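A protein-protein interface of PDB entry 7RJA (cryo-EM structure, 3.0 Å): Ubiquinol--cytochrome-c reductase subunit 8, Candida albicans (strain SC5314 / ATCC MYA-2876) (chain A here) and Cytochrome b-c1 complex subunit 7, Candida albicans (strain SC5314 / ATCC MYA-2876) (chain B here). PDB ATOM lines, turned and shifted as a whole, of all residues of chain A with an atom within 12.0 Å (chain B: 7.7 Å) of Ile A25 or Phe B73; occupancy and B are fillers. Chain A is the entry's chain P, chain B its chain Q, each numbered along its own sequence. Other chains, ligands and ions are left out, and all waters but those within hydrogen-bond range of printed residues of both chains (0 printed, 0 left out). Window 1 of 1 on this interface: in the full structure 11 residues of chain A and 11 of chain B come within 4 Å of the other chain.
The backbone carbonyl oxygen (O) of Pro A20 is in hydrogen-bond range of the side-chain amide nitrogen (ND2) of Asn B72, 3.5 Å away.
ND2 of Asn B72 sits at hydrogen-bond distance from O of Lys A21, 3.2 Å away.
The backbone carbonyl oxygen (O) of Asn B68 sits close to the side-chain amide oxygen (OD1) of Asn B72 (3.1 Å).
The backbone carbonyl oxygen of Phe B73 sits at hydrogen-bond distance from the side-chain hydroxyl of Thr B77, at 3.1 Å.
The side-chain hydroxyl (OH) of Tyr A24 lies close to the side-chain amino group (NZ) of Lys A23, at 3.1 Å.
Pro A20 touches Asn B68 (CB to OD1, 3.4 Å).
ND2 of Asn B68 touches O of Lys A21, 3.9 Å away.
O of Lys A21 touches CE1 of Tyr B69 (3.1 Å).
Gln A22 touches Asn B72 (CB to ND2, 3.3 Å).
Tyr B69 touches Lys A23.
Tyr A24 touches Tyr B69.
Ile A25 touches Phe B73 (CD1 to CA, 3.8 Å).
CG2 of Ile A25 touches CD2 of Leu B76, 3.6 Å away.
Phe B73 touches just one residue of chain A: Ile A25 (3.8 Å).
No residue of chain A comes within 4 Å of Ser B70.
Of chain A, only Pro A20, Lys A21 and Gln A22 come within 4 Å of Asn B72.
No residue of chain A comes within 4 Å of Arg B74.
Of chain A, only Ile A25 (3.6 Å) comes within 4 Å of Leu B76.
No residue of chain A comes within 4 Å of Thr B77.
Of the printed residues of chain B, Gln A22 touches Asn B72 (3.3 Å).
Of the printed residues of chain B, Lys A21 touches Asn B68 (3.9 Å), Tyr B69 (3.1 Å) and Asn B72 (3.2 Å).
Of the printed residues of chain B, Lys A23 touches Tyr B69 (3.6 Å).
Hydrophobic or aromatic side chains of chain A within 4 Å of the printed part of chain B: Pro A20, Tyr A24 and Ile A25.
Of the 18 printed residues of chain B, 5 touch a printed residue of chain A.
Hydrophobic or aromatic side chains of chain B within 4 Å of the printed part of chain A: Tyr B69, Phe B73 and Leu B76.
Among the printed residues, 10 pairs touch across the chains.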
ATOM      1  N   SER A  19     -15.987 -19.057  17.919  1.00  0.00           N
ATOM      2  CA  SER A  19     -15.076 -19.160  16.794  1.00  0.00           C
ATOM      3  C   SER A  19     -15.058 -20.594  16.270  1.00  0.00           C
ATOM      4  O   SER A  19     -15.194 -21.540  17.050  1.00  0.00           O
ATOM      5  CB  SER A  19     -13.667 -18.745  17.207  1.00  0.00           C
ATOM      6  OG  SER A  19     -13.136 -19.645  18.161  1.00  0.00           O
ATOM      7  N   PRO A  20     -14.895 -20.791  14.965  1.00  0.00           N
ATOM      8  CA  PRO A  20     -14.751 -22.155  14.447  1.00  0.00           C
ATOM      9  C   PRO A  20     -13.475 -22.793  14.968  1.00  0.00           C
ATOM     10  O   PRO A  20     -12.558 -22.119  15.441  1.00  0.00           O
ATOM     11  CB  PRO A  20     -14.707 -21.965  12.927  1.00  0.00           C
ATOM     12  CG  PRO A  20     -15.249 -20.603  12.684  1.00  0.00           C
ATOM     13  CD  PRO A  20     -14.890 -19.797  13.882  1.00  0.00           C
ATOM     14  N   LYS A  21     -13.426 -24.120  14.894  1.00  0.00           N
ATOM     15  CA  LYS A  21     -12.219 -24.835  15.280  1.00  0.00           C
ATOM     16  C   LYS A  21     -11.011 -24.189  14.627  1.00  0.00           C
ATOM     17  O   LYS A  21     -10.884 -24.190  13.400  1.00  0.00           O
ATOM     18  CB  LYS A  21     -12.316 -26.303  14.861  1.00  0.00           C
ATOM     19  CG  LYS A  21     -13.382 -27.121  15.575  1.00  0.00           C
ATOM     20  CD  LYS A  21     -13.384 -26.878  17.078  1.00  0.00           C
ATOM     21  CE  LYS A  21     -14.247 -27.891  17.823  1.00  0.00           C
ATOM     22  NZ  LYS A  21     -14.018 -29.291  17.369  1.00  0.00           N
ATOM     23  N   GLN A  22     -10.122 -23.639  15.446  1.00  0.00           N
ATOM     24  CA  GLN A  22      -8.963 -22.906  14.960  1.00  0.00           C
ATOM     25  C   GLN A  22      -7.713 -23.691  15.322  1.00  0.00           C
ATOM     26  O   GLN A  22      -7.591 -24.191  16.443  1.00  0.00           O
ATOM     27  CB  GLN A  22      -8.925 -21.493  15.545  1.00  0.00           C
ATOM     28  CG  GLN A  22      -7.713 -20.681  15.142  1.00  0.00           C
ATOM     29  CD  GLN A  22      -7.549 -19.438  15.985  1.00  0.00           C
ATOM     30  OE1 GLN A  22      -8.438 -19.076  16.747  1.00  0.00           O
ATOM     31  NE2 GLN A  22      -6.409 -18.772  15.846  1.00  0.00           N
ATOM     32  N   LYS A  23      -6.791 -23.800  14.371  1.00  0.00           N
ATOM     33  CA  LYS A  23      -5.696 -24.749  14.486  1.00  0.00           C
ATOM     34  C   LYS A  23      -4.611 -24.348  13.502  1.00  0.00           C
ATOM     35  O   LYS A  23      -4.893 -23.719  12.480  1.00  0.00           O
ATOM     36  CB  LYS A  23      -6.195 -26.171  14.206  1.00  0.00           C
ATOM     37  CG  LYS A  23      -5.249 -27.296  14.574  1.00  0.00           C
ATOM     38  CD  LYS A  23      -5.975 -28.631  14.481  1.00  0.00           C
ATOM     39  CE  LYS A  23      -5.130 -29.789  14.973  1.00  0.00           C
ATOM     40  NZ  LYS A  23      -4.032 -30.117  14.035  1.00  0.00           N
ATOM     41  N   TYR A  24      -3.370 -24.702  13.826  1.00  0.00           N
ATOM     42  CA  TYR A  24      -2.194 -24.432  13.005  1.00  0.00           C
ATOM     43  C   TYR A  24      -1.776 -22.969  12.999  1.00  0.00           C
ATOM     44  O   TYR A  24      -0.904 -22.594  12.208  1.00  0.00           O
ATOM     45  CB  TYR A  24      -2.397 -24.875  11.553  1.00  0.00           C
ATOM     46  CG  TYR A  24      -2.811 -26.312  11.397  1.00  0.00           C
ATOM     47  CD1 TYR A  24      -2.079 -27.329  11.982  1.00  0.00           C
ATOM     48  CD2 TYR A  24      -3.929 -26.655  10.657  1.00  0.00           C
ATOM     49  CE1 TYR A  24      -2.448 -28.643  11.838  1.00  0.00           C
ATOM     50  CE2 TYR A  24      -4.307 -27.967  10.508  1.00  0.00           C
ATOM     51  CZ  TYR A  24      -3.564 -28.958  11.101  1.00  0.00           C
ATOM     52  OH  TYR A  24      -3.938 -30.270  10.956  1.00  0.00           O
ATOM     53  N   ILE A  25      -2.356 -22.130  13.848  1.00  0.00           N
ATOM     54  CA  ILE A  25      -2.026 -20.710  13.900  1.00  0.00           C
ATOM     55  C   ILE A  25      -1.215 -20.459  15.159  1.00  0.00           C
ATOM     56  O   ILE A  25      -1.651 -20.795  16.266  1.00  0.00           O
ATOM     57  CB  ILE A  25      -3.283 -19.830  13.864  1.00  0.00           C
ATOM     58  CG1 ILE A  25      -4.007 -20.011  12.530  1.00  0.00           C
ATOM     59  CG2 ILE A  25      -2.916 -18.375  14.068  1.00  0.00           C
ATOM     60  CD1 ILE A  25      -5.381 -19.398  12.486  1.00  0.00           C
ATOM     61  N   THR A  26      -0.034 -19.874  14.990  1.00  0.00           N
ATOM     62  CA  THR A  26       0.852 -19.525  16.090  1.00  0.00           C
ATOM     63  C   THR A  26       0.912 -18.011  16.210  1.00  0.00           C
ATOM     64  O   THR A  26       1.111 -17.320  15.208  1.00  0.00           O
ATOM     65  CB  THR A  26       2.255 -20.084  15.859  1.00  0.00           C
ATOM     66  OG1 THR A  26       2.178 -21.493  15.620  1.00  0.00           O
ATOM     67  CG2 THR A  26       3.133 -19.832  17.062  1.00  0.00           C
ATOM     68  N   GLN A  27       0.739 -17.498  17.424  1.00  0.00           N
ATOM     69  CA  GLN A  27       0.773 -16.064  17.681  1.00  0.00           C
ATOM     70  C   GLN A  27       1.973 -15.746  18.556  1.00  0.00           C
ATOM     71  O   GLN A  27       2.115 -16.309  19.644  1.00  0.00           O
ATOM     72  CB  GLN A  27      -0.511 -15.590  18.360  1.00  0.00           C
ATOM     73  CG  GLN A  27      -1.781 -16.141  17.750  1.00  0.00           C
ATOM     74  CD  GLN A  27      -3.021 -15.569  18.395  1.00  0.00           C
ATOM     75  OE1 GLN A  27      -2.974 -14.508  19.016  1.00  0.00           O
ATOM     76  NE2 GLN A  27      -4.140 -16.266  18.249  1.00  0.00           N
ATOM     77  N   TYR A  28       2.821 -14.837  18.090  1.00  0.00           N
ATOM     78  CA  TYR A  28       3.990 -14.394  18.830  1.00  0.00           C
ATOM     79  C   TYR A  28       3.801 -12.949  19.268  1.00  0.00           C
ATOM     80  O   TYR A  28       3.154 -12.157  18.580  1.00  0.00           O
ATOM     81  CB  TYR A  28       5.258 -14.501  17.983  1.00  0.00           C
ATOM     82  CG  TYR A  28       5.498 -15.862  17.382  1.00  0.00           C
ATOM     83  CD1 TYR A  28       5.999 -16.899  18.146  1.00  0.00           C
ATOM     84  CD2 TYR A  28       5.238 -16.103  16.046  1.00  0.00           C
ATOM     85  CE1 TYR A  28       6.224 -18.139  17.597  1.00  0.00           C
ATOM     86  CE2 TYR A  28       5.460 -17.337  15.490  1.00  0.00           C
ATOM     87  CZ  TYR A  28       5.954 -18.352  16.269  1.00  0.00           C
ATOM     88  OH  TYR A  28       6.177 -19.589  15.718  1.00  0.00           O
ATOM     89  N   THR A  29       4.366 -12.613  20.423  1.00  0.00           N
ATOM     90  CA  THR A  29       4.369 -11.236  20.897  1.00  0.00           C
ATOM     91  C   THR A  29       5.447 -11.102  21.959  1.00  0.00           C
ATOM     92  O   THR A  29       5.972 -12.094  22.464  1.00  0.00           O
ATOM     93  CB  THR A  29       3.001 -10.822  21.442  1.00  0.00           C
ATOM     94  OG1 THR A  29       3.043  -9.451  21.851  1.00  0.00           O
ATOM     95  CG2 THR A  29       2.607 -11.683  22.620  1.00  0.00           C
ATOM     96  N   MET B  41      -6.280  -6.315   2.690  1.00  0.00           N
ATOM     97  CA  MET B  41      -6.221  -6.756   4.075  1.00  0.00           C
ATOM     98  C   MET B  41      -6.206  -8.272   4.202  1.00  0.00           C
ATOM     99  O   MET B  41      -6.404  -8.792   5.304  1.00  0.00           O
ATOM    100  CB  MET B  41      -7.397  -6.177   4.858  1.00  0.00           C
ATOM    101  CG  MET B  41      -7.335  -4.674   5.007  1.00  0.00           C
ATOM    102  SD  MET B  41      -8.769  -4.008   5.858  1.00  0.00           S
ATOM    103  CE  MET B  41      -8.475  -4.602   7.515  1.00  0.00           C
ATOM    104  N   GLY B  42      -5.986  -8.989   3.105  1.00  0.00           N
ATOM    105  CA  GLY B  42      -5.905 -10.430   3.137  1.00  0.00           C
ATOM    106  C   GLY B  42      -7.231 -11.148   3.062  1.00  0.00           C
ATOM    107  O   GLY B  42      -7.243 -12.382   3.009  1.00  0.00           O
ATOM    108  N   LEU B  43      -8.346 -10.426   3.050  1.00  0.00           N
ATOM    109  CA  LEU B  43      -9.657 -11.057   3.050  1.00  0.00           C
ATOM    110  C   LEU B  43     -10.083 -11.419   1.637  1.00  0.00           C
ATOM    111  O   LEU B  43      -9.971 -10.606   0.717  1.00  0.00           O
ATOM    112  CB  LEU B  43     -10.695 -10.126   3.672  1.00  0.00           C
ATOM    113  CG  LEU B  43     -10.496  -9.783   5.143  1.00  0.00           C
ATOM    114  CD1 LEU B  43     -11.253  -8.525   5.502  1.00  0.00           C
ATOM    115  CD2 LEU B  43     -10.941 -10.936   6.013  1.00  0.00           C
ATOM    116  N   ASP B  47     -15.071 -13.927   3.116  1.00  0.00           N
ATOM    117  CA  ASP B  47     -14.792 -13.632   4.512  1.00  0.00           C
ATOM    118  C   ASP B  47     -15.663 -12.492   5.017  1.00  0.00           C
ATOM    119  O   ASP B  47     -16.023 -12.465   6.198  1.00  0.00           O
ATOM    120  CB  ASP B  47     -13.320 -13.287   4.679  1.00  0.00           C
ATOM    121  CG  ASP B  47     -12.418 -14.344   4.100  1.00  0.00           C
ATOM    122  OD1 ASP B  47     -12.768 -15.537   4.196  1.00  0.00           O
ATOM    123  OD2 ASP B  47     -11.364 -13.990   3.536  1.00  0.00           O
ATOM    124  N   LEU B  67     -10.144 -25.362   4.424  1.00  0.00           N
ATOM    125  CA  LEU B  67     -10.778 -24.080   4.145  1.00  0.00           C
ATOM    126  C   LEU B  67     -11.127 -23.359   5.435  1.00  0.00           C
ATOM    127  O   LEU B  67     -10.996 -22.136   5.526  1.00  0.00           O
ATOM    128  CB  LEU B  67     -12.027 -24.274   3.287  1.00  0.00           C
ATOM    129  CG  LEU B  67     -11.809 -24.777   1.860  1.00  0.00           C
ATOM    130  CD1 LEU B  67     -13.125 -24.843   1.111  1.00  0.00           C
ATOM    131  CD2 LEU B  67     -10.829 -23.887   1.122  1.00  0.00           C
ATOM    132  N   ASN B  68     -11.573 -24.101   6.448  1.00  0.00           N
ATOM    133  CA  ASN B  68     -11.921 -23.474   7.716  1.00  0.00           C
ATOM    134  C   ASN B  68     -10.708 -22.815   8.355  1.00  0.00           C
ATOM    135  O   ASN B  68     -10.784 -21.672   8.821  1.00  0.00           O
ATOM    136  CB  ASN B  68     -12.523 -24.512   8.657  1.00  0.00           C
ATOM    137  CG  ASN B  68     -13.115 -23.894   9.895  1.00  0.00           C
ATOM    138  OD1 ASN B  68     -13.066 -22.680  10.078  1.00  0.00           O
ATOM    139  ND2 ASN B  68     -13.683 -24.726  10.756  1.00  0.00           N
ATOM    140  N   TYR B  69      -9.572 -23.513   8.380  1.00  0.00           N
ATOM    141  CA  TYR B  69      -8.377 -22.938   8.987  1.00  0.00           C
ATOM    142  C   TYR B  69      -7.846 -21.771   8.166  1.00  0.00           C
ATOM    143  O   TYR B  69      -7.396 -20.765   8.726  1.00  0.00           O
ATOM    144  CB  TYR B  69      -7.307 -24.011   9.153  1.00  0.00           C
ATOM    145  CG  TYR B  69      -7.740 -25.171  10.015  1.00  0.00           C
ATOM    146  CD1 TYR B  69      -8.535 -24.971  11.131  1.00  0.00           C
ATOM    147  CD2 TYR B  69      -7.358 -26.464   9.711  1.00  0.00           C
ATOM    148  CE1 TYR B  69      -8.934 -26.025  11.917  1.00  0.00           C
ATOM    149  CE2 TYR B  69      -7.754 -27.523  10.491  1.00  0.00           C
ATOM    150  CZ  TYR B  69      -8.540 -27.298  11.594  1.00  0.00           C
ATOM    151  OH  TYR B  69      -8.937 -28.354  12.376  1.00  0.00           O
ATOM    152  N   SER B  70      -7.885 -21.882   6.837  1.00  0.00           N
ATOM    153  CA  SER B  70      -7.457 -20.764   6.008  1.00  0.00           C
ATOM    154  C   SER B  70      -8.323 -19.541   6.262  1.00  0.00           C
ATOM    155  O   SER B  70      -7.815 -18.421   6.373  1.00  0.00           O
ATOM    156  CB  SER B  70      -7.500 -21.160   4.535  1.00  0.00           C
ATOM    157  OG  SER B  70      -7.080 -20.092   3.708  1.00  0.00           O
ATOM    158  N   ARG B  71      -9.639 -19.738   6.364  1.00  0.00           N
ATOM    159  CA  ARG B  71     -10.537 -18.631   6.664  1.00  0.00           C
ATOM    160  C   ARG B  71     -10.228 -18.030   8.023  1.00  0.00           C
ATOM    161  O   ARG B  71     -10.230 -16.804   8.185  1.00  0.00           O
ATOM    162  CB  ARG B  71     -11.984 -19.112   6.613  1.00  0.00           C
ATOM    163  CG  ARG B  71     -13.000 -18.057   6.976  1.00  0.00           C
ATOM    164  CD  ARG B  71     -14.401 -18.624   6.976  1.00  0.00           C
ATOM    165  NE  ARG B  71     -15.394 -17.572   7.132  1.00  0.00           N
ATOM    166  CZ  ARG B  71     -15.872 -17.157   8.297  1.00  0.00           C
ATOM    167  NH1 ARG B  71     -15.463 -17.681   9.440  1.00  0.00           N
ATOM    168  NH2 ARG B  71     -16.776 -16.182   8.316  1.00  0.00           N
ATOM    169  N   ASN B  72      -9.973 -18.876   9.020  1.00  0.00           N
ATOM    170  CA  ASN B  72      -9.643 -18.365  10.345  1.00  0.00           C
ATOM    171  C   ASN B  72      -8.398 -17.497  10.291  1.00  0.00           C
ATOM    172  O   ASN B  72      -8.359 -16.408  10.874  1.00  0.00           O
ATOM    173  CB  ASN B  72      -9.442 -19.523  11.318  1.00  0.00           C
ATOM    174  CG  ASN B  72     -10.738 -20.163  11.730  1.00  0.00           C
ATOM    175  OD1 ASN B  72     -11.788 -19.894  11.152  1.00  0.00           O
ATOM    176  ND2 ASN B  72     -10.677 -21.022  12.734  1.00  0.00           N
ATOM    177  N   PHE B  73      -7.366 -17.961   9.589  1.00  0.00           N
ATOM    178  CA  PHE B  73      -6.134 -17.183   9.536  1.00  0.00           C
ATOM    179  C   PHE B  73      -6.333 -15.886   8.768  1.00  0.00           C
ATOM    180  O   PHE B  73      -5.781 -14.851   9.147  1.00  0.00           O
ATOM    181  CB  PHE B  73      -5.003 -17.985   8.908  1.00  0.00           C
ATOM    182  CG  PHE B  73      -3.731 -17.204   8.777  1.00  0.00           C
ATOM    183  CD1 PHE B  73      -3.067 -16.755   9.901  1.00  0.00           C
ATOM    184  CD2 PHE B  73      -3.208 -16.906   7.535  1.00  0.00           C
ATOM    185  CE1 PHE B  73      -1.904 -16.035   9.789  1.00  0.00           C
ATOM    186  CE2 PHE B  73      -2.043 -16.183   7.421  1.00  0.00           C
ATOM    187  CZ  PHE B  73      -1.393 -15.747   8.549  1.00  0.00           C
ATOM    188  N   ARG B  74      -7.099 -15.916   7.679  1.00  0.00           N
ATOM    189  CA  ARG B  74      -7.328 -14.683   6.935  1.00  0.00           C
ATOM    190  C   ARG B  74      -8.105 -13.674   7.767  1.00  0.00           C
ATOM    191  O   ARG B  74      -7.796 -12.478   7.747  1.00  0.00           O
ATOM    192  CB  ARG B  74      -8.055 -14.978   5.627  1.00  0.00           C
ATOM    193  CG  ARG B  74      -7.120 -15.365   4.502  1.00  0.00           C
ATOM    194  CD  ARG B  74      -7.862 -15.552   3.202  1.00  0.00           C
ATOM    195  NE  ARG B  74      -8.329 -16.923   3.042  1.00  0.00           N
ATOM    196  CZ  ARG B  74      -9.570 -17.331   3.265  1.00  0.00           C
ATOM    197  NH1 ARG B  74     -10.507 -16.500   3.682  1.00  0.00           N
ATOM    198  NH2 ARG B  74      -9.877 -18.609   3.066  1.00  0.00           N
ATOM    199  N   ILE B  75      -9.109 -14.133   8.513  1.00  0.00           N
ATOM    200  CA  ILE B  75      -9.861 -13.226   9.374  1.00  0.00           C
ATOM    201  C   ILE B  75      -8.964 -12.661  10.466  1.00  0.00           C
ATOM    202  O   ILE B  75      -9.025 -11.468  10.785  1.00  0.00           O
ATOM    203  CB  ILE B  75     -11.083 -13.946   9.964  1.00  0.00           C
ATOM    204  CG1 ILE B  75     -12.135 -14.159   8.876  1.00  0.00           C
ATOM    205  CG2 ILE B  75     -11.641 -13.155  11.134  1.00  0.00           C
ATOM    206  CD1 ILE B  75     -13.295 -15.022   9.298  1.00  0.00           C
ATOM    207  N   LEU B  76      -8.125 -13.507  11.064  1.00  0.00           N
ATOM    208  CA  LEU B  76      -7.213 -13.030  12.096  1.00  0.00           C
ATOM    209  C   LEU B  76      -6.239 -12.002  11.535  1.00  0.00           C
ATOM    210  O   LEU B  76      -5.958 -10.984  12.178  1.00  0.00           O
ATOM    211  CB  LEU B  76      -6.461 -14.213  12.697  1.00  0.00           C
ATOM    212  CG  LEU B  76      -5.371 -13.896  13.712  1.00  0.00           C
ATOM    213  CD1 LEU B  76      -5.962 -13.230  14.927  1.00  0.00           C
ATOM    214  CD2 LEU B  76      -4.646 -15.166  14.102  1.00  0.00           C
ATOM    215  N   THR B  77      -5.715 -12.253  10.336  1.00  0.00           N
ATOM    216  CA  THR B  77      -4.810 -11.300   9.707  1.00  0.00           C
ATOM    217  C   THR B  77      -5.513  -9.983   9.423  1.00  0.00           C
ATOM    218  O   THR B  77      -4.934  -8.910   9.612  1.00  0.00           O
ATOM    219  CB  THR B  77      -4.249 -11.888   8.415  1.00  0.00           C
ATOM    220  OG1 THR B  77      -3.383 -12.984   8.723  1.00  0.00           O
ATOM    221  CG2 THR B  77      -3.474 -10.839   7.648  1.00  0.00           C
ATOM    222  N   ALA B  78      -6.758 -10.044   8.952  1.00  0.00           N
ATOM    223  CA  ALA B  78      -7.506  -8.818   8.711  1.00  0.00           C
ATOM    224  C   ALA B  78      -7.701  -8.038  10.000  1.00  0.00           C
ATOM    225  O   ALA B  78      -7.565  -6.809  10.020  1.00  0.00           O
ATOM    226  CB  ALA B  78      -8.855  -9.144   8.080  1.00  0.00           C
ATOM    227  N   HIS B  79      -8.037  -8.734  11.085  1.00  0.00           N
ATOM    228  CA  HIS B  79      -8.207  -8.055  12.363  1.00  0.00           C
ATOM    229  C   HIS B  79      -6.913  -7.395  12.802  1.00  0.00           C
ATOM    230  O   HIS B  79      -6.915  -6.248  13.256  1.00  0.00           O
ATOM    231  CB  HIS B  79      -8.688  -9.037  13.426  1.00  0.00           C
ATOM    232  CG  HIS B  79     -10.169  -9.232  13.435  1.00  0.00           C
ATOM    233  ND1 HIS B  79     -10.826  -9.968  12.475  1.00  0.00           N
ATOM    234  CD2 HIS B  79     -11.123  -8.776  14.277  1.00  0.00           C
ATOM    235  CE1 HIS B  79     -12.120  -9.966  12.732  1.00  0.00           C
ATOM    236  NE2 HIS B  79     -12.328  -9.248  13.819  1.00  0.00           N
ATOM    237  N   GLN B  80      -5.791  -8.099  12.664  1.00  0.00           N
ATOM    238  CA  GLN B  80      -4.509  -7.518  13.046  1.00  0.00           C
ATOM    239  C   GLN B  80      -4.176  -6.301  12.195  1.00  0.00           C
ATOM    240  O   GLN B  80      -3.660  -5.302  12.705  1.00  0.00           O
ATOM    241  CB  GLN B  80      -3.408  -8.566  12.931  1.00  0.00           C
ATOM    242  CG  GLN B  80      -2.024  -8.062  13.285  1.00  0.00           C
ATOM    243  CD  GLN B  80      -1.936  -7.545  14.698  1.00  0.00           C
ATOM    244  OE1 GLN B  80      -2.753  -7.889  15.549  1.00  0.00           O
ATOM    245  NE2 GLN B  80      -0.941  -6.710  14.960  1.00  0.00           N
